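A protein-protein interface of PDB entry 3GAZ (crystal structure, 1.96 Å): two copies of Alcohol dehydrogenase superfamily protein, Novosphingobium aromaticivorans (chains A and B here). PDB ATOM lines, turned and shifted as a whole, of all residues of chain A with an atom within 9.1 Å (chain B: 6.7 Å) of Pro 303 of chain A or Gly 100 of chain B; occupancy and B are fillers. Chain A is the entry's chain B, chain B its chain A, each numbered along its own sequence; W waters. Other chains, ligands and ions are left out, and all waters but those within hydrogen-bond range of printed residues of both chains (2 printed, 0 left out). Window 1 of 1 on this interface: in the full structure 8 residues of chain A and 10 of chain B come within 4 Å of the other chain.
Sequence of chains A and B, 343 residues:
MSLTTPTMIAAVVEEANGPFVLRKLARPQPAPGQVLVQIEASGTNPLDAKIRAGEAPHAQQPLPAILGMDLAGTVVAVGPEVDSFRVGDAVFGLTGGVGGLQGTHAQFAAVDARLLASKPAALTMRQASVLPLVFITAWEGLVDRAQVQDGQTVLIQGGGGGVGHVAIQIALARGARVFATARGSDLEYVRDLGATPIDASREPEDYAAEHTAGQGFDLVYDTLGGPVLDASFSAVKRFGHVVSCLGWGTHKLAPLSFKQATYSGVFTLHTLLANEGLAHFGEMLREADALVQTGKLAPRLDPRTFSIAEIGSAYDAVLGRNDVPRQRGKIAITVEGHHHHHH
No position is printed for both chains.
Of the 7 pairs that touch across the chains among the printed residues, none has its exchanged pair printed and touching as well.
Water W1 lies within hydrogen-bond range of the backbone carbonyl oxygen (O) of Leu 273 of chain B, the side-chain amide nitrogen (NE2) of Gln 60 of chain B and the backbone NH (N) of Thr 305 of chain A.
Water W2 bridges O of Gly 100 of chain B and NE of Arg 328 of chain A.
NE2 of Gln 60 of chain B lies within hydrogen-bond range of O of Pro 303 of chain A, 3.2 Å away.
The side-chain amide oxygen (OE1) of Gln 60 of chain B is in hydrogen-bond range of the side-chain hydroxyl (OG1) of Thr 305 of chain A.
Printed residues of chain A that touch a printed residue of chain B: Pro 303, Arg 304 and Thr 305.
Hydrophobic or aromatic side chains of chain A within 4 Å of the printed part of chain B: Pro 303.
Of the 12 printed residues of chain B, 5 touch a printed residue of chain A.
Printed residues of chain B that touch a printed residue of chain A: Gln 60, Pro 62, Gly 99, Gly 100 and Leu 273.
Hydrophobic or aromatic side chains of chain B within 4 Å of the printed part of chain A: Pro 62.
Along chain B the printed residues that touch a printed residue of chain A span positions 60 to 273.
The backbone carbonyl oxygen (O) of Arg 304 of chain A sits at hydrogen-bond distance from the guanidinium group (NH1) of Arg 126 of chain A (3.1 Å).
The backbone NH (N) of Gly 100 of chain B is in hydrogen-bond range of the side-chain amide oxygen (OE1) of Gln 61 of chain B.
The side-chain carboxylate (OD2) of Asp 302 of chain A is in salt-bridge range of the guanidinium group (NH2) of Arg 304 of chain A (2.9 Å).
The backbone carbonyl oxygen (O) of Pro 325 of chain A is in hydrogen-bond range of the guanidinium group (NH1) of Arg 304 of chain A (3.1 Å).
The backbone NH of Gly 100 of chain B is in hydrogen-bond range of the backbone carbonyl oxygen of Gln 60 of chain B, at 3.3 Å.
OE1 of Gln 61 of chain B is in hydrogen-bond range of N of Gly 99 of chain B (3.4 Å).
Pro 62 of chain B touches Pro 303 of chain A.
CB of Pro 303 of chain A touches C of Gly 99 of chain B, at 3.96 Å.
Pro 303 of chain A touches Gly 100 of chain B.
Arg 304 of chain A touches Gln 60 of chain B.
CG of Arg 304 of chain A touches O of Leu 273 of chain B (3.7 Å).
Printed residues of chain B within 4 Å of Thr 305 of chain A: Gln 60 (3.4 Å).
Printed residues of chain A within 4 Å of Gln 60 of chain B: Pro 303 (3.2 Å), Arg 304 (3.8 Å) and Thr 305 (3.4 Å).
Of chain A, only Pro 303 comes within 4 Å of Gly 99 of chain B.
The nearest residue of chain B that does not touch Pro 303 of chain A is Gln 61 of chain B (5.1 Å).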
ATOM      1  N   ARG A 126     -10.615  -9.883 -20.385  1.00  0.00           N
ATOM      2  CA  ARG A 126     -11.004 -11.246 -20.020  1.00  0.00           C
ATOM      3  C   ARG A 126     -12.455 -11.271 -19.523  1.00  0.00           C
ATOM      4  O   ARG A 126     -13.268 -12.074 -19.990  1.00  0.00           O
ATOM      5  CB  ARG A 126     -10.062 -11.794 -18.934  1.00  0.00           C
ATOM      6  CG  ARG A 126      -8.806 -12.483 -19.488  1.00  0.00           C
ATOM      7  CD  ARG A 126      -7.747 -12.734 -18.410  1.00  0.00           C
ATOM      8  NE  ARG A 126      -8.280 -13.357 -17.195  1.00  0.00           N
ATOM      9  CZ  ARG A 126      -8.658 -14.630 -17.087  1.00  0.00           C
ATOM     10  NH1 ARG A 126      -8.569 -15.454 -18.123  1.00  0.00           N
ATOM     11  NH2 ARG A 126      -9.126 -15.082 -15.930  1.00  0.00           N
ATOM     12  N   ARG A 300     -18.919 -14.119 -14.174  1.00  0.00           N
ATOM     13  CA  ARG A 300     -18.210 -15.062 -13.328  1.00  0.00           C
ATOM     14  C   ARG A 300     -17.069 -15.544 -14.206  1.00  0.00           C
ATOM     15  O   ARG A 300     -17.283 -16.240 -15.200  1.00  0.00           O
ATOM     16  CB  ARG A 300     -19.095 -16.238 -12.928  1.00  0.00           C
ATOM     17  CG  ARG A 300     -18.517 -17.006 -11.754  1.00  0.00           C
ATOM     18  CD  ARG A 300     -19.336 -18.227 -11.393  1.00  0.00           C
ATOM     19  NE  ARG A 300     -18.889 -18.796 -10.125  1.00  0.00           N
ATOM     20  CZ  ARG A 300     -19.240 -19.996  -9.677  1.00  0.00           C
ATOM     21  NH1 ARG A 300     -20.040 -20.765 -10.401  1.00  0.00           N
ATOM     22  NH2 ARG A 300     -18.802 -20.419  -8.498  1.00  0.00           N
ATOM     23  N   LEU A 301     -15.856 -15.158 -13.839  1.00  0.00           N
ATOM     24  CA  LEU A 301     -14.667 -15.501 -14.601  1.00  0.00           C
ATOM     25  C   LEU A 301     -13.696 -16.368 -13.815  1.00  0.00           C
ATOM     26  O   LEU A 301     -13.199 -15.960 -12.768  1.00  0.00           O
ATOM     27  CB  LEU A 301     -13.965 -14.210 -15.040  1.00  0.00           C
ATOM     28  CG  LEU A 301     -12.604 -14.272 -15.744  1.00  0.00           C
ATOM     29  CD1 LEU A 301     -12.746 -14.924 -17.106  1.00  0.00           C
ATOM     30  CD2 LEU A 301     -12.055 -12.855 -15.898  1.00  0.00           C
ATOM     31  N   ASP A 302     -13.434 -17.568 -14.321  1.00  0.00           N
ATOM     32  CA  ASP A 302     -12.485 -18.462 -13.667  1.00  0.00           C
ATOM     33  C   ASP A 302     -11.139 -17.721 -13.709  1.00  0.00           C
ATOM     34  O   ASP A 302     -10.781 -17.141 -14.735  1.00  0.00           O
ATOM     35  CB  ASP A 302     -12.408 -19.786 -14.427  1.00  0.00           C
ATOM     36  CG  ASP A 302     -11.514 -20.804 -13.743  1.00  0.00           C
ATOM     37  OD1 ASP A 302     -10.291 -20.563 -13.667  1.00  0.00           O
ATOM     38  OD2 ASP A 302     -12.037 -21.843 -13.279  1.00  0.00           O
ATOM     39  N   PRO A 303     -10.392 -17.715 -12.585  1.00  0.00           N
ATOM     40  CA  PRO A 303      -9.085 -17.059 -12.414  1.00  0.00           C
ATOM     41  C   PRO A 303      -7.952 -17.538 -13.313  1.00  0.00           C
ATOM     42  O   PRO A 303      -6.956 -16.835 -13.492  1.00  0.00           O
ATOM     43  CB  PRO A 303      -8.761 -17.311 -10.938  1.00  0.00           C
ATOM     44  CG  PRO A 303     -10.101 -17.475 -10.303  1.00  0.00           C
ATOM     45  CD  PRO A 303     -10.826 -18.321 -11.314  1.00  0.00           C
ATOM     46  N   ARG A 304      -8.089 -18.736 -13.865  1.00  0.00           N
ATOM     47  CA  ARG A 304      -7.050 -19.294 -14.726  1.00  0.00           C
ATOM     48  C   ARG A 304      -6.912 -18.540 -16.043  1.00  0.00           C
ATOM     49  O   ARG A 304      -7.889 -18.015 -16.574  1.00  0.00           O
ATOM     50  CB  ARG A 304      -7.338 -20.768 -15.012  1.00  0.00           C
ATOM     51  CG  ARG A 304      -7.019 -21.700 -13.854  1.00  0.00           C
ATOM     52  CD  ARG A 304      -7.498 -23.116 -14.144  1.00  0.00           C
ATOM     53  NE  ARG A 304      -8.941 -23.250 -13.968  1.00  0.00           N
ATOM     54  CZ  ARG A 304      -9.616 -24.388 -14.106  1.00  0.00           C
ATOM     55  NH1 ARG A 304      -8.978 -25.507 -14.432  1.00  0.00           N
ATOM     56  NH2 ARG A 304     -10.931 -24.414 -13.903  1.00  0.00           N
ATOM     57  N   THR A 305      -5.686 -18.484 -16.556  1.00  0.00           N
ATOM     58  CA  THR A 305      -5.407 -17.816 -17.819  1.00  0.00           C
ATOM     59  C   THR A 305      -4.884 -18.834 -18.824  1.00  0.00           C
ATOM     60  O   THR A 305      -4.280 -19.843 -18.449  1.00  0.00           O
ATOM     61  CB  THR A 305      -4.346 -16.722 -17.659  1.00  0.00           C
ATOM     62  OG1 THR A 305      -3.180 -17.288 -17.050  1.00  0.00           O
ATOM     63  CG2 THR A 305      -4.880 -15.575 -16.804  1.00  0.00           C
ATOM     64  N   PHE A 306      -5.128 -18.558 -20.101  1.00  0.00           N
ATOM     65  CA  PHE A 306      -4.695 -19.426 -21.190  1.00  0.00           C
ATOM     66  C   PHE A 306      -4.322 -18.546 -22.374  1.00  0.00           C
ATOM     67  O   PHE A 306      -5.107 -17.696 -22.789  1.00  0.00           O
ATOM     68  CB  PHE A 306      -5.835 -20.364 -21.604  1.00  0.00           C
ATOM     69  CG  PHE A 306      -6.348 -21.222 -20.486  1.00  0.00           C
ATOM     70  CD1 PHE A 306      -5.755 -22.448 -20.203  1.00  0.00           C
ATOM     71  CD2 PHE A 306      -7.403 -20.783 -19.689  1.00  0.00           C
ATOM     72  CE1 PHE A 306      -6.204 -23.235 -19.137  1.00  0.00           C
ATOM     73  CE2 PHE A 306      -7.860 -21.560 -18.618  1.00  0.00           C
ATOM     74  CZ  PHE A 306      -7.258 -22.787 -18.342  1.00  0.00           C
ATOM     75  N   PRO A 325      -9.571 -29.429 -13.017  1.00  0.00           N
ATOM     76  CA  PRO A 325     -10.806 -28.987 -12.365  1.00  0.00           C
ATOM     77  C   PRO A 325     -11.732 -28.290 -13.358  1.00  0.00           C
ATOM     78  O   PRO A 325     -11.276 -27.553 -14.229  1.00  0.00           O
ATOM     79  CB  PRO A 325     -10.304 -28.034 -11.284  1.00  0.00           C
ATOM     80  CG  PRO A 325      -8.948 -28.581 -10.949  1.00  0.00           C
ATOM     81  CD  PRO A 325      -8.386 -28.906 -12.310  1.00  0.00           C
ATOM     82  N   ARG A 326     -13.030 -28.535 -13.229  1.00  0.00           N
ATOM     83  CA  ARG A 326     -14.009 -27.914 -14.113  1.00  0.00           C
ATOM     84  C   ARG A 326     -13.969 -26.397 -13.913  1.00  0.00           C
ATOM     85  O   ARG A 326     -13.603 -25.912 -12.842  1.00  0.00           O
ATOM     86  CB  ARG A 326     -15.409 -28.444 -13.787  1.00  0.00           C
ATOM     87  CG  ARG A 326     -16.533 -27.788 -14.576  1.00  0.00           C
ATOM     88  CD  ARG A 326     -16.948 -28.593 -15.801  1.00  0.00           C
ATOM     89  NE  ARG A 326     -17.912 -27.850 -16.611  1.00  0.00           N
ATOM     90  CZ  ARG A 326     -18.583 -28.346 -17.649  1.00  0.00           C
ATOM     91  NH1 ARG A 326     -18.410 -29.608 -18.023  1.00  0.00           N
ATOM     92  NH2 ARG A 326     -19.423 -27.568 -18.322  1.00  0.00           N
ATOM     93  N   GLN A 327     -14.346 -25.647 -14.943  1.00  0.00           N
ATOM     94  CA  GLN A 327     -14.352 -24.198 -14.831  1.00  0.00           C
ATOM     95  C   GLN A 327     -15.275 -23.755 -13.705  1.00  0.00           C
ATOM     96  O   GLN A 327     -16.325 -24.356 -13.468  1.00  0.00           O
ATOM     97  CB  GLN A 327     -14.804 -23.543 -16.148  1.00  0.00           C
ATOM     98  CG  GLN A 327     -16.117 -24.068 -16.713  1.00  0.00           C
ATOM     99  CD  GLN A 327     -16.633 -23.224 -17.873  1.00  0.00           C
ATOM    100  OE1 GLN A 327     -15.869 -22.814 -18.746  1.00  0.00           O
ATOM    101  NE2 GLN A 327     -17.940 -22.976 -17.892  1.00  0.00           N
ATOM    102  N   ARG A 328     -14.859 -22.706 -13.009  1.00  0.00           N
ATOM    103  CA  ARG A 328     -15.628 -22.126 -11.914  1.00  0.00           C
ATOM    104  C   ARG A 328     -15.852 -20.717 -12.449  1.00  0.00           C
ATOM    105  O   ARG A 328     -15.063 -19.798 -12.218  1.00  0.00           O
ATOM    106  CB  ARG A 328     -14.784 -22.126 -10.637  1.00  0.00           C
ATOM    107  CG  ARG A 328     -15.585 -22.085  -9.347  1.00  0.00           C
ATOM    108  CD  ARG A 328     -14.732 -22.556  -8.177  1.00  0.00           C
ATOM    109  NE  ARG A 328     -14.872 -21.694  -7.006  1.00  0.00           N
ATOM    110  CZ  ARG A 328     -15.987 -21.564  -6.293  1.00  0.00           C
ATOM    111  NH1 ARG A 328     -17.077 -22.243  -6.626  1.00  0.00           N
ATOM    112  NH2 ARG A 328     -16.014 -20.747  -5.246  1.00  0.00           N
ATOM    113  N   GLY A 329     -16.949 -20.563 -13.177  1.00  0.00           N
ATOM    114  CA  GLY A 329     -17.222 -19.304 -13.826  1.00  0.00           C
ATOM    115  C   GLY A 329     -16.781 -19.666 -15.233  1.00  0.00           C
ATOM    116  O   GLY A 329     -16.550 -20.848 -15.505  1.00  0.00           O
ATOM    117  N   LYS A 330     -16.634 -18.697 -16.124  1.00  0.00           N
ATOM    118  CA  LYS A 330     -16.240 -19.043 -17.479  1.00  0.00           C
ATOM    119  C   LYS A 330     -14.750 -18.866 -17.757  1.00  0.00           C
ATOM    120  O   LYS A 330     -14.043 -18.151 -17.044  1.00  0.00           O
ATOM    121  CB  LYS A 330     -17.090 -18.253 -18.480  1.00  0.00           C
ATOM    122  CG  LYS A 330     -18.591 -18.582 -18.379  1.00  0.00           C
ATOM    123  CD  LYS A 330     -19.444 -17.729 -19.307  1.00  0.00           C
ATOM    124  CE  LYS A 330     -18.997 -17.862 -20.757  1.00  0.00           C
ATOM    125  NZ  LYS A 330     -19.039 -19.277 -21.212  1.00  0.00           N
ATOM    126  N   ILE A 331     -14.289 -19.538 -18.808  1.00  0.00           N
ATOM    127  CA  ILE A 331     -12.893 -19.519 -19.227  1.00  0.00           C
ATOM    128  C   ILE A 331     -12.638 -18.547 -20.378  1.00  0.00           C
ATOM    129  O   ILE A 331     -13.286 -18.640 -21.422  1.00  0.00           O
ATOM    130  CB  ILE A 331     -12.461 -20.924 -19.710  1.00  0.00           C
ATOM    131  CG1 ILE A 331     -12.644 -21.948 -18.586  1.00  0.00           C
ATOM    132  CG2 ILE A 331     -11.028 -20.887 -20.215  1.00  0.00           C
ATOM    133  CD1 ILE A 331     -11.699 -21.753 -17.412  1.00  0.00           C
ATOM    134  N   ALA A 332     -11.689 -17.630 -20.197  1.00  0.00           N
ATOM    135  CA  ALA A 332     -11.342 -16.683 -21.255  1.00  0.00           C
ATOM    136  C   ALA A 332      -9.913 -16.960 -21.717  1.00  0.00           C
ATOM    137  O   ALA A 332      -9.041 -17.296 -20.910  1.00  0.00           O
ATOM    138  CB  ALA A 332     -11.466 -15.236 -20.757  1.00  0.00           C
ATOM    139  N   THR A 334      -6.517 -15.501 -23.414  1.00  0.00           N
ATOM    140  CA  THR A 334      -5.831 -14.242 -23.654  1.00  0.00           C
ATOM    141  C   THR A 334      -5.075 -14.355 -24.968  1.00  0.00           C
ATOM    142  O   THR A 334      -4.023 -14.996 -25.045  1.00  0.00           O
ATOM    143  CB  THR A 334      -4.842 -13.897 -22.519  1.00  0.00           C
ATOM    144  OG1 THR A 334      -5.566 -13.734 -21.291  1.00  0.00           O
ATOM    145  CG2 THR A 334      -4.096 -12.597 -22.837  1.00  0.00           C
ATOM    146  N   ALA B  59      -0.511 -14.544  -8.503  1.00  0.00           N
ATOM    147  CA  ALA B  59      -1.196 -15.607  -7.772  1.00  0.00           C
ATOM    148  C   ALA B  59      -2.543 -15.975  -8.384  1.00  0.00           C
ATOM    149  O   ALA B  59      -3.059 -17.066  -8.151  1.00  0.00           O
ATOM    150  CB  ALA B  59      -1.382 -15.201  -6.310  1.00  0.00           C
ATOM    151  N   GLN B  60      -3.108 -15.063  -9.168  1.00  0.00           N
ATOM    152  CA  GLN B  60      -4.394 -15.305  -9.809  1.00  0.00           C
ATOM    153  C   GLN B  60      -5.415 -15.831  -8.797  1.00  0.00           C
ATOM    154  O   GLN B  60      -6.101 -16.827  -9.041  1.00  0.00           O
ATOM    155  CB  GLN B  60      -4.221 -16.302 -10.964  1.00  0.00           C
ATOM    156  CG  GLN B  60      -3.196 -15.841 -12.000  1.00  0.00           C
ATOM    157  CD  GLN B  60      -3.005 -16.815 -13.155  1.00  0.00           C
ATOM    158  OE1 GLN B  60      -2.071 -16.672 -13.938  1.00  0.00           O
ATOM    159  NE2 GLN B  60      -3.888 -17.803 -13.267  1.00  0.00           N
ATOM    160  N   GLN B  61      -5.508 -15.149  -7.660  1.00  0.00           N
ATOM    161  CA  GLN B  61      -6.445 -15.525  -6.606  1.00  0.00           C
ATOM    162  C   GLN B  61      -7.327 -14.326  -6.246  1.00  0.00           C
ATOM    163  O   GLN B  61      -7.114 -13.661  -5.225  1.00  0.00           O
ATOM    164  CB  GLN B  61      -5.690 -15.995  -5.356  1.00  0.00           C
ATOM    165  CG  GLN B  61      -6.595 -16.562  -4.263  1.00  0.00           C
ATOM    166  CD  GLN B  61      -6.992 -18.011  -4.523  1.00  0.00           C
ATOM    167  OE1 GLN B  61      -7.045 -18.453  -5.666  1.00  0.00           O
ATOM    168  NE2 GLN B  61      -7.285 -18.750  -3.455  1.00  0.00           N
ATOM    169  N   PRO B  62      -8.327 -14.026  -7.091  1.00  0.00           N
ATOM    170  CA  PRO B  62      -9.210 -12.894  -6.803  1.00  0.00           C
ATOM    171  C   PRO B  62     -10.109 -13.180  -5.602  1.00  0.00           C
ATOM    172  O   PRO B  62     -10.359 -14.339  -5.262  1.00  0.00           O
ATOM    173  CB  PRO B  62      -9.998 -12.734  -8.100  1.00  0.00           C
ATOM    174  CG  PRO B  62     -10.107 -14.160  -8.592  1.00  0.00           C
ATOM    175  CD  PRO B  62      -8.708 -14.692  -8.350  1.00  0.00           C
ATOM    176  N   GLY B  97      -4.953 -22.072  -2.568  1.00  0.00           N
ATOM    177  CA  GLY B  97      -4.709 -20.709  -2.131  1.00  0.00           C
ATOM    178  C   GLY B  97      -4.353 -19.789  -3.284  1.00  0.00           C
ATOM    179  O   GLY B  97      -4.235 -18.575  -3.105  1.00  0.00           O
ATOM    180  N   VAL B  98      -4.187 -20.370  -4.467  1.00  0.00           N
ATOM    181  CA  VAL B  98      -3.853 -19.609  -5.672  1.00  0.00           C
ATOM    182  C   VAL B  98      -4.618 -20.141  -6.886  1.00  0.00           C
ATOM    183  O   VAL B  98      -5.169 -21.241  -6.855  1.00  0.00           O
ATOM    184  CB  VAL B  98      -2.350 -19.694  -5.994  1.00  0.00           C
ATOM    185  CG1 VAL B  98      -1.531 -19.149  -4.834  1.00  0.00           C
ATOM    186  CG2 VAL B  98      -1.967 -21.144  -6.297  1.00  0.00           C
ATOM    187  N   GLY B  99      -4.644 -19.348  -7.956  1.00  0.00           N
ATOM    188  CA  GLY B  99      -5.313 -19.751  -9.181  1.00  0.00           C
ATOM    189  C   GLY B  99      -6.768 -20.162  -9.051  1.00  0.00           C
ATOM    190  O   GLY B  99      -7.263 -20.954  -9.856  1.00  0.00           O
ATOM    191  N   GLY B 100      -7.458 -19.626  -8.047  1.00  0.00           N
ATOM    192  CA  GLY B 100      -8.857 -19.965  -7.855  1.00  0.00           C
ATOM    193  C   GLY B 100      -9.091 -21.218  -7.022  1.00  0.00           C
ATOM    194  O   GLY B 100     -10.237 -21.574  -6.735  1.00  0.00           O
ATOM    195  N   LEU B 101      -8.015 -21.893  -6.637  1.00  0.00           N
ATOM    196  CA  LEU B 101      -8.123 -23.102  -5.825  1.00  0.00           C
ATOM    197  C   LEU B 101      -8.458 -22.721  -4.386  1.00  0.00           C
ATOM    198  O   LEU B 101      -7.907 -21.750  -3.854  1.00  0.00           O
ATOM    199  CB  LEU B 101      -6.801 -23.878  -5.853  1.00  0.00           C
ATOM    200  CG  LEU B 101      -6.408 -24.536  -7.183  1.00  0.00           C
ATOM    201  CD1 LEU B 101      -4.947 -24.932  -7.145  1.00  0.00           C
ATOM    202  CD2 LEU B 101      -7.290 -25.757  -7.436  1.00  0.00           C
ATOM    203  N   GLN B 102      -9.364 -23.470  -3.760  1.00  0.00           N
ATOM    204  CA  GLN B 102      -9.729 -23.182  -2.377  1.00  0.00           C
ATOM    205  C   GLN B 102      -8.486 -23.198  -1.490  1.00  0.00           C
ATOM    206  O   GLN B 102      -7.649 -24.093  -1.602  1.00  0.00           O
ATOM    207  CB  GLN B 102     -10.719 -24.215  -1.831  1.00  0.00           C
ATOM    208  CG  GLN B 102     -11.088 -23.927  -0.382  1.00  0.00           C
ATOM    209  CD  GLN B 102     -11.597 -25.143   0.361  1.00  0.00           C
ATOM    210  OE1 GLN B 102     -12.645 -25.695   0.035  1.00  0.00           O
ATOM    211  NE2 GLN B 102     -10.850 -25.567   1.375  1.00  0.00           N
ATOM    212  N   GLY B 103      -8.381 -22.216  -0.599  1.00  0.00           N
ATOM    213  CA  GLY B 103      -7.240 -22.144   0.299  1.00  0.00           C
ATOM    214  C   GLY B 103      -7.335 -23.147   1.433  1.00  0.00           C
ATOM    215  O   GLY B 103      -8.333 -23.866   1.557  1.00  0.00           O
ATOM    216  N   LEU B 273      -1.236 -23.182 -11.086  1.00  0.00           N
ATOM    217  CA  LEU B 273      -1.970 -22.219 -11.915  1.00  0.00           C
ATOM    218  C   LEU B 273      -2.336 -22.766 -13.284  1.00  0.00           C
ATOM    219  O   LEU B 273      -3.348 -22.389 -13.863  1.00  0.00           O
ATOM    220  CB  LEU B 273      -1.139 -20.940 -12.093  1.00  0.00           C
ATOM    221  CG  LEU B 273      -0.843 -20.156 -10.802  1.00  0.00           C
ATOM    222  CD1 LEU B 273       0.151 -19.061 -11.091  1.00  0.00           C
ATOM    223  CD2 LEU B 273      -2.114 -19.554 -10.267  1.00  0.00           C
HETATM  224  O   HOH W   1      -3.480 -19.903 -15.158  1.00  0.00           O
HETATM  225  O   HOH W   2     -12.257 -20.954  -8.810  1.00  0.00           O
